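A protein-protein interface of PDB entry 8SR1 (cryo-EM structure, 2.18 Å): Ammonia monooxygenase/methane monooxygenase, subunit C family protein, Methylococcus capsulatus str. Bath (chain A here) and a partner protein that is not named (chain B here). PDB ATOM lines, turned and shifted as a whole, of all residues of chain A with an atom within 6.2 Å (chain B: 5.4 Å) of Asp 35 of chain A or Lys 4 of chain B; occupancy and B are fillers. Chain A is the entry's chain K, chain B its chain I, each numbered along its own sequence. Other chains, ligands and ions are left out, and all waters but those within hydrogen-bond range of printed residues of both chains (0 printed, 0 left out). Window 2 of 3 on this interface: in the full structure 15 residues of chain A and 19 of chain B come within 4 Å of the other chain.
Leu 34 of chain A touches His 1 of chain B. OG of Ser 5 of chain B touches OG of Ser 36 of chain A (3.6 Å). Lys 4 of chain B touches Phe 37 of chain A. CE2 of Phe 37 of chain A touches OG of Ser 5 of chain B, 3.0 Å away. CZ of Phe 37 of chain A touches NE of Arg 343 of chain B, at 3.4 Å.
NZ of Lys 4 of chain B is in hydrogen-bond range of O of Val 341 of chain B, at 3.3 Å. The backbone carbonyl oxygen (O) of Ser 5 of chain B sits at hydrogen-bond distance from the guanidinium group (NH2) of Arg 343 of chain B (3.3 Å). O of Arg 343 of chain B sits at hydrogen-bond distance from NH2 of Arg 11 of chain B (3.2 Å). OD1 of Asp 35 of chain A sits close to N of Phe 37 of chain A, 3.2 Å away. The backbone NH of Ala 38 of chain A lies within hydrogen-bond range of the side-chain carboxylate of Asp 35 of chain A (3.5 Å). The side-chain hydroxyl (OG) of Ser 36 of chain A sits at hydrogen-bond distance from the side-chain carboxylate (OD2) of Asp 122 of chain A (3.0 Å).
NZ of Lys 4 of chain B lies within salt-bridge range of OD2 of Asp 35 of chain A (3.6 Å). The side-chain hydroxyl (OG) of Ser 5 of chain B is in hydrogen-bond range of the side-chain carboxylate (OD1) of Asp 122 of chain A, at 2.8 Å. The side-chain carboxylate of Asp 122 of chain A lies close to the backbone carbonyl oxygen of His 1 of chain B, at 3.3 Å. The backbone carbonyl oxygen (O) of Gly 2 of chain B lies close to the side-chain carboxylate (OD1) of Asp 122 of chain A, at 3.0 Å. OD1 of Asp 122 of chain A lies close to O of Glu 3 of chain B (3.4 Å).
Lys 4 of chain B touches two residues of chain A. Of the printed residues of chain B, Ser 36 of chain A touches Ser 5 (3.6 Å). Printed residues of chain A within 4 Å of Arg 343 of chain B: Phe 37 (3.4 Å). Of the printed residues of chain A, His 1 of chain B touches Leu 34 (3.3 Å) and Asp 122 (3.3 Å). Pro 39 of chain A touches none of the printed residues of chain B. The nearest residue of chain B that does not touch Asp 35 of chain A is His 1 of chain B (4.2 Å). The nearest residue of chain A that does not touch Lys 4 of chain B is Asp 122 of chain A (5.2 Å). The nearest printed residue of chain B that does not touch Asp 122 of chain A is Lys 4 of chain B (5.2 Å).
Printed residues of chain B that touch a printed residue of chain A: His 1, Gly 2, Glu 3, Lys 4, Ser 5 and Arg 343. Hydrophobic or aromatic side chains of chain B that line the printed part of chain A: His 1. Of the 12 printed residues of chain A, 5 touch a printed residue of chain B.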
ATOM      1  N   ALA A  32      -6.197 -12.548 -11.198  1.00  0.00           N
ATOM      2  CA  ALA A  32      -6.154 -11.831 -12.480  1.00  0.00           C
ATOM      3  C   ALA A  32      -4.734 -11.710 -13.024  1.00  0.00           C
ATOM      4  O   ALA A  32      -4.123 -10.642 -13.028  1.00  0.00           O
ATOM      5  CB  ALA A  32      -6.815 -10.452 -12.389  1.00  0.00           C
ATOM      6  N   GLY A  33      -4.223 -12.838 -13.523  1.00  0.00           N
ATOM      7  CA  GLY A  33      -2.866 -12.939 -14.023  1.00  0.00           C
ATOM      8  C   GLY A  33      -2.280 -14.333 -13.932  1.00  0.00           C
ATOM      9  O   GLY A  33      -1.182 -14.581 -14.436  1.00  0.00           O
ATOM     10  N   LEU A  34      -3.004 -15.262 -13.307  1.00  0.00           N
ATOM     11  CA  LEU A  34      -2.591 -16.662 -13.324  1.00  0.00           C
ATOM     12  C   LEU A  34      -3.236 -17.422 -14.482  1.00  0.00           C
ATOM     13  O   LEU A  34      -2.584 -18.231 -15.149  1.00  0.00           O
ATOM     14  CB  LEU A  34      -2.921 -17.327 -11.986  1.00  0.00           C
ATOM     15  CG  LEU A  34      -1.874 -17.191 -10.881  1.00  0.00           C
ATOM     16  CD1 LEU A  34      -1.995 -18.336  -9.890  1.00  0.00           C
ATOM     17  CD2 LEU A  34      -0.475 -17.146 -11.470  1.00  0.00           C
ATOM     18  N   ASP A  35      -4.523 -17.178 -14.726  1.00  0.00           N
ATOM     19  CA  ASP A  35      -5.248 -17.866 -15.787  1.00  0.00           C
ATOM     20  C   ASP A  35      -5.336 -16.962 -17.010  1.00  0.00           C
ATOM     21  O   ASP A  35      -6.015 -15.932 -16.981  1.00  0.00           O
ATOM     22  CB  ASP A  35      -6.640 -18.264 -15.305  1.00  0.00           C
ATOM     23  CG  ASP A  35      -7.445 -18.986 -16.368  1.00  0.00           C
ATOM     24  OD1 ASP A  35      -6.846 -19.495 -17.339  1.00  0.00           O
ATOM     25  OD2 ASP A  35      -8.687 -19.060 -16.227  1.00  0.00           O
ATOM     26  N   SER A  36      -4.663 -17.355 -18.091  1.00  0.00           N
ATOM     27  CA  SER A  36      -4.583 -16.531 -19.291  1.00  0.00           C
ATOM     28  C   SER A  36      -5.874 -16.516 -20.100  1.00  0.00           C
ATOM     29  O   SER A  36      -5.992 -15.709 -21.026  1.00  0.00           O
ATOM     30  CB  SER A  36      -3.428 -17.008 -20.178  1.00  0.00           C
ATOM     31  OG  SER A  36      -3.771 -18.202 -20.860  1.00  0.00           O
ATOM     32  N   PHE A  37      -6.835 -17.381 -19.786  1.00  0.00           N
ATOM     33  CA  PHE A  37      -8.118 -17.397 -20.473  1.00  0.00           C
ATOM     34  C   PHE A  37      -9.252 -16.836 -19.623  1.00  0.00           C
ATOM     35  O   PHE A  37     -10.402 -16.845 -20.069  1.00  0.00           O
ATOM     36  CB  PHE A  37      -8.455 -18.820 -20.928  1.00  0.00           C
ATOM     37  CG  PHE A  37      -7.677 -19.265 -22.131  1.00  0.00           C
ATOM     38  CD1 PHE A  37      -8.019 -18.820 -23.396  1.00  0.00           C
ATOM     39  CD2 PHE A  37      -6.600 -20.123 -22.000  1.00  0.00           C
ATOM     40  CE1 PHE A  37      -7.302 -19.222 -24.505  1.00  0.00           C
ATOM     41  CE2 PHE A  37      -5.881 -20.531 -23.103  1.00  0.00           C
ATOM     42  CZ  PHE A  37      -6.232 -20.081 -24.358  1.00  0.00           C
ATOM     43  N   ALA A  38      -8.956 -16.355 -18.421  1.00  0.00           N
ATOM     44  CA  ALA A  38      -9.957 -15.704 -17.597  1.00  0.00           C
ATOM     45  C   ALA A  38     -10.239 -14.298 -18.116  1.00  0.00           C
ATOM     46  O   ALA A  38      -9.352 -13.638 -18.660  1.00  0.00           O
ATOM     47  CB  ALA A  38      -9.487 -15.649 -16.148  1.00  0.00           C
ATOM     48  N   PRO A  39     -11.479 -13.817 -17.970  1.00  0.00           N
ATOM     49  CA  PRO A  39     -11.790 -12.461 -18.450  1.00  0.00           C
ATOM     50  C   PRO A  39     -10.986 -11.374 -17.758  1.00  0.00           C
ATOM     51  O   PRO A  39     -10.627 -10.382 -18.403  1.00  0.00           O
ATOM     52  CB  PRO A  39     -13.292 -12.324 -18.166  1.00  0.00           C
ATOM     53  CG  PRO A  39     -13.555 -13.288 -17.064  1.00  0.00           C
ATOM     54  CD  PRO A  39     -12.630 -14.446 -17.303  1.00  0.00           C
ATOM     55  N   GLU A  40     -10.687 -11.532 -16.467  1.00  0.00           N
ATOM     56  CA  GLU A  40      -9.905 -10.542 -15.740  1.00  0.00           C
ATOM     57  C   GLU A  40      -8.465 -10.449 -16.232  1.00  0.00           C
ATOM     58  O   GLU A  40      -7.857  -9.373 -16.140  1.00  0.00           O
ATOM     59  CB  GLU A  40      -9.938 -10.862 -14.246  1.00  0.00           C
ATOM     60  CG  GLU A  40      -9.381 -12.230 -13.891  1.00  0.00           C
ATOM     61  CD  GLU A  40     -10.449 -13.302 -13.828  1.00  0.00           C
ATOM     62  OE1 GLU A  40     -11.485 -13.152 -14.507  1.00  0.00           O
ATOM     63  OE2 GLU A  40     -10.252 -14.294 -13.095  1.00  0.00           O
ATOM     64  N   PHE A  41      -7.913 -11.543 -16.764  1.00  0.00           N
ATOM     65  CA  PHE A  41      -6.599 -11.478 -17.387  1.00  0.00           C
ATOM     66  C   PHE A  41      -6.586 -10.516 -18.560  1.00  0.00           C
ATOM     67  O   PHE A  41      -5.639  -9.741 -18.706  1.00  0.00           O
ATOM     68  CB  PHE A  41      -6.159 -12.870 -17.842  1.00  0.00           C
ATOM     69  CG  PHE A  41      -4.795 -12.901 -18.475  1.00  0.00           C
ATOM     70  CD1 PHE A  41      -3.660 -13.070 -17.696  1.00  0.00           C
ATOM     71  CD2 PHE A  41      -4.642 -12.763 -19.844  1.00  0.00           C
ATOM     72  CE1 PHE A  41      -2.408 -13.102 -18.272  1.00  0.00           C
ATOM     73  CE2 PHE A  41      -3.390 -12.795 -20.426  1.00  0.00           C
ATOM     74  CZ  PHE A  41      -2.272 -12.963 -19.636  1.00  0.00           C
ATOM     75  N   GLU A  42      -7.632 -10.530 -19.386  1.00  0.00           N
ATOM     76  CA  GLU A  42      -7.739  -9.589 -20.488  1.00  0.00           C
ATOM     77  C   GLU A  42      -7.768  -8.139 -20.026  1.00  0.00           C
ATOM     78  O   GLU A  42      -7.125  -7.292 -20.657  1.00  0.00           O
ATOM     79  CB  GLU A  42      -8.991  -9.883 -21.314  1.00  0.00           C
ATOM     80  CG  GLU A  42      -8.710 -10.251 -22.760  1.00  0.00           C
ATOM     81  CD  GLU A  42      -8.503  -9.033 -23.639  1.00  0.00           C
ATOM     82  OE1 GLU A  42      -8.876  -7.921 -23.211  1.00  0.00           O
ATOM     83  OE2 GLU A  42      -7.966  -9.190 -24.755  1.00  0.00           O
ATOM     84  N   ASP A 122       1.462 -20.829 -19.171  1.00  0.00           N
ATOM     85  CA  ASP A 122       0.129 -20.839 -19.851  1.00  0.00           C
ATOM     86  C   ASP A 122       0.086 -20.194 -21.246  1.00  0.00           C
ATOM     87  O   ASP A 122      -0.670 -20.720 -22.075  1.00  0.00           O
ATOM     88  CB  ASP A 122      -0.928 -20.158 -18.983  1.00  0.00           C
ATOM     89  CG  ASP A 122      -2.232 -20.934 -18.914  1.00  0.00           C
ATOM     90  OD1 ASP A 122      -2.180 -22.173 -19.051  1.00  0.00           O
ATOM     91  OD2 ASP A 122      -3.286 -20.292 -18.732  1.00  0.00           O
ATOM     92  N   HIS B   1      -4.048 -24.041 -13.153  1.00  0.00           N
ATOM     93  CA  HIS B   1      -4.330 -22.701 -13.660  1.00  0.00           C
ATOM     94  C   HIS B   1      -3.520 -22.690 -14.946  1.00  0.00           C
ATOM     95  O   HIS B   1      -3.748 -21.803 -15.785  1.00  0.00           O
ATOM     96  CB  HIS B   1      -3.864 -21.569 -12.712  1.00  0.00           C
ATOM     97  CG  HIS B   1      -4.926 -20.978 -11.836  1.00  0.00           C
ATOM     98  ND1 HIS B   1      -5.899 -21.781 -11.301  1.00  0.00           N
ATOM     99  CD2 HIS B   1      -5.174 -19.717 -11.368  1.00  0.00           C
ATOM    100  CE1 HIS B   1      -6.728 -21.046 -10.590  1.00  0.00           C
ATOM    101  NE2 HIS B   1      -6.287 -19.804 -10.569  1.00  0.00           N
ATOM    102  N   GLY B   2      -2.614 -23.672 -15.071  1.00  0.00           N
ATOM    103  CA  GLY B   2      -1.769 -23.803 -16.272  1.00  0.00           C
ATOM    104  C   GLY B   2      -2.379 -24.736 -17.303  1.00  0.00           C
ATOM    105  O   GLY B   2      -1.691 -25.033 -18.292  1.00  0.00           O
ATOM    106  N   GLU B   3      -3.566 -25.284 -17.053  1.00  0.00           N
ATOM    107  CA  GLU B   3      -4.219 -26.090 -18.124  1.00  0.00           C
ATOM    108  C   GLU B   3      -5.222 -25.171 -18.841  1.00  0.00           C
ATOM    109  O   GLU B   3      -5.108 -23.936 -18.639  1.00  0.00           O
ATOM    110  CB  GLU B   3      -4.744 -27.430 -17.585  1.00  0.00           C
ATOM    111  CG  GLU B   3      -6.194 -27.433 -17.156  1.00  0.00           C
ATOM    112  CD  GLU B   3      -6.477 -26.455 -16.036  1.00  0.00           C
ATOM    113  OE1 GLU B   3      -6.101 -26.749 -14.890  1.00  0.00           O
ATOM    114  OE2 GLU B   3      -7.048 -25.393 -16.329  1.00  0.00           O
ATOM    115  N   LYS B   4      -6.129 -25.715 -19.661  1.00  0.00           N
ATOM    116  CA  LYS B   4      -7.050 -24.878 -20.488  1.00  0.00           C
ATOM    117  C   LYS B   4      -6.232 -24.210 -21.598  1.00  0.00           C
ATOM    118  O   LYS B   4      -6.843 -23.522 -22.419  1.00  0.00           O
ATOM    119  CB  LYS B   4      -7.789 -23.811 -19.670  1.00  0.00           C
ATOM    120  CG  LYS B   4      -8.966 -24.298 -18.843  1.00  0.00           C
ATOM    121  CD  LYS B   4      -9.205 -23.454 -17.610  1.00  0.00           C
ATOM    122  CE  LYS B   4     -10.626 -22.948 -17.497  1.00  0.00           C
ATOM    123  NZ  LYS B   4     -10.723 -21.515 -17.863  1.00  0.00           N
ATOM    124  N   SER B   5      -4.907 -24.388 -21.602  1.00  0.00           N
ATOM    125  CA  SER B   5      -4.013 -23.812 -22.638  1.00  0.00           C
ATOM    126  C   SER B   5      -3.290 -24.957 -23.344  1.00  0.00           C
ATOM    127  O   SER B   5      -2.946 -24.784 -24.520  1.00  0.00           O
ATOM    128  CB  SER B   5      -3.036 -22.847 -22.029  1.00  0.00           C
ATOM    129  OG  SER B   5      -3.716 -21.779 -21.396  1.00  0.00           O
ATOM    130  N   GLN B   6      -3.074 -26.083 -22.654  1.00  0.00           N
ATOM    131  CA  GLN B   6      -2.479 -27.227 -23.316  1.00  0.00           C
ATOM    132  C   GLN B   6      -3.450 -27.830 -24.326  1.00  0.00           C
ATOM    133  O   GLN B   6      -4.663 -27.610 -24.273  1.00  0.00           O
ATOM    134  CB  GLN B   6      -2.060 -28.280 -22.293  1.00  0.00           C
ATOM    135  CG  GLN B   6      -1.586 -27.705 -20.976  1.00  0.00           C
ATOM    136  CD  GLN B   6      -1.160 -28.780 -19.997  1.00  0.00           C
ATOM    137  OE1 GLN B   6      -1.948 -29.217 -19.160  1.00  0.00           O
ATOM    138  NE2 GLN B   6       0.092 -29.205 -20.096  1.00  0.00           N
ATOM    139  N   ARG B  11      -4.229 -33.351 -23.194  1.00  0.00           N
ATOM    140  CA  ARG B  11      -4.841 -33.444 -21.874  1.00  0.00           C
ATOM    141  C   ARG B  11      -5.733 -34.672 -21.766  1.00  0.00           C
ATOM    142  O   ARG B  11      -5.846 -35.267 -20.687  1.00  0.00           O
ATOM    143  CB  ARG B  11      -5.641 -32.181 -21.570  1.00  0.00           C
ATOM    144  CG  ARG B  11      -4.794 -31.005 -21.127  1.00  0.00           C
ATOM    145  CD  ARG B  11      -5.662 -29.842 -20.696  1.00  0.00           C
ATOM    146  NE  ARG B  11      -6.141 -29.075 -21.839  1.00  0.00           N
ATOM    147  CZ  ARG B  11      -7.365 -28.584 -21.953  1.00  0.00           C
ATOM    148  NH1 ARG B  11      -8.268 -28.751 -20.999  1.00  0.00           N
ATOM    149  NH2 ARG B  11      -7.697 -27.910 -23.051  1.00  0.00           N
ATOM    150  N   VAL B 341     -15.340 -24.118 -21.456  1.00  0.00           N
ATOM    151  CA  VAL B 341     -14.561 -23.334 -20.503  1.00  0.00           C
ATOM    152  C   VAL B 341     -13.124 -23.833 -20.435  1.00  0.00           C
ATOM    153  O   VAL B 341     -12.181 -23.033 -20.467  1.00  0.00           O
ATOM    154  CB  VAL B 341     -15.237 -23.359 -19.120  1.00  0.00           C
ATOM    155  CG1 VAL B 341     -14.259 -22.942 -18.037  1.00  0.00           C
ATOM    156  CG2 VAL B 341     -16.461 -22.457 -19.113  1.00  0.00           C
ATOM    157  N   TYR B 342     -12.923 -25.148 -20.352  1.00  0.00           N
ATOM    158  CA  TYR B 342     -11.594 -25.738 -20.323  1.00  0.00           C
ATOM    159  C   TYR B 342     -11.059 -26.021 -21.720  1.00  0.00           C
ATOM    160  O   TYR B 342     -10.076 -26.751 -21.865  1.00  0.00           O
ATOM    161  CB  TYR B 342     -11.604 -27.008 -19.474  1.00  0.00           C
ATOM    162  CG  TYR B 342     -11.484 -26.716 -18.000  1.00  0.00           C
ATOM    163  CD1 TYR B 342     -12.570 -26.244 -17.276  1.00  0.00           C
ATOM    164  CD2 TYR B 342     -10.280 -26.899 -17.330  1.00  0.00           C
ATOM    165  CE1 TYR B 342     -12.464 -25.962 -15.930  1.00  0.00           C
ATOM    166  CE2 TYR B 342     -10.167 -26.623 -15.984  1.00  0.00           C
ATOM    167  CZ  TYR B 342     -11.261 -26.155 -15.288  1.00  0.00           C
ATOM    168  OH  TYR B 342     -11.150 -25.882 -13.946  1.00  0.00           O
ATOM    169  N   ARG B 343     -11.688 -25.404 -22.728  1.00  0.00           N
ATOM    170  CA  ARG B 343     -11.207 -25.498 -24.134  1.00  0.00           C
ATOM    171  C   ARG B 343     -11.010 -26.948 -24.583  1.00  0.00           C
ATOM    172  O   ARG B 343      -9.990 -27.225 -25.247  1.00  0.00           O
ATOM    173  CB  ARG B 343      -9.944 -24.645 -24.296  1.00  0.00           C
ATOM    174  CG  ARG B 343     -10.208 -23.149 -24.226  1.00  0.00           C
ATOM    175  CD  ARG B 343      -9.270 -22.404 -25.150  1.00  0.00           C
ATOM    176  NE  ARG B 343      -7.939 -22.944 -24.942  1.00  0.00           N
ATOM    177  CZ  ARG B 343      -7.012 -23.121 -25.873  1.00  0.00           C
ATOM    178  NH1 ARG B 343      -7.237 -22.775 -27.128  1.00  0.00           N
ATOM    179  NH2 ARG B 343      -5.847 -23.632 -25.526  1.00  0.00           N
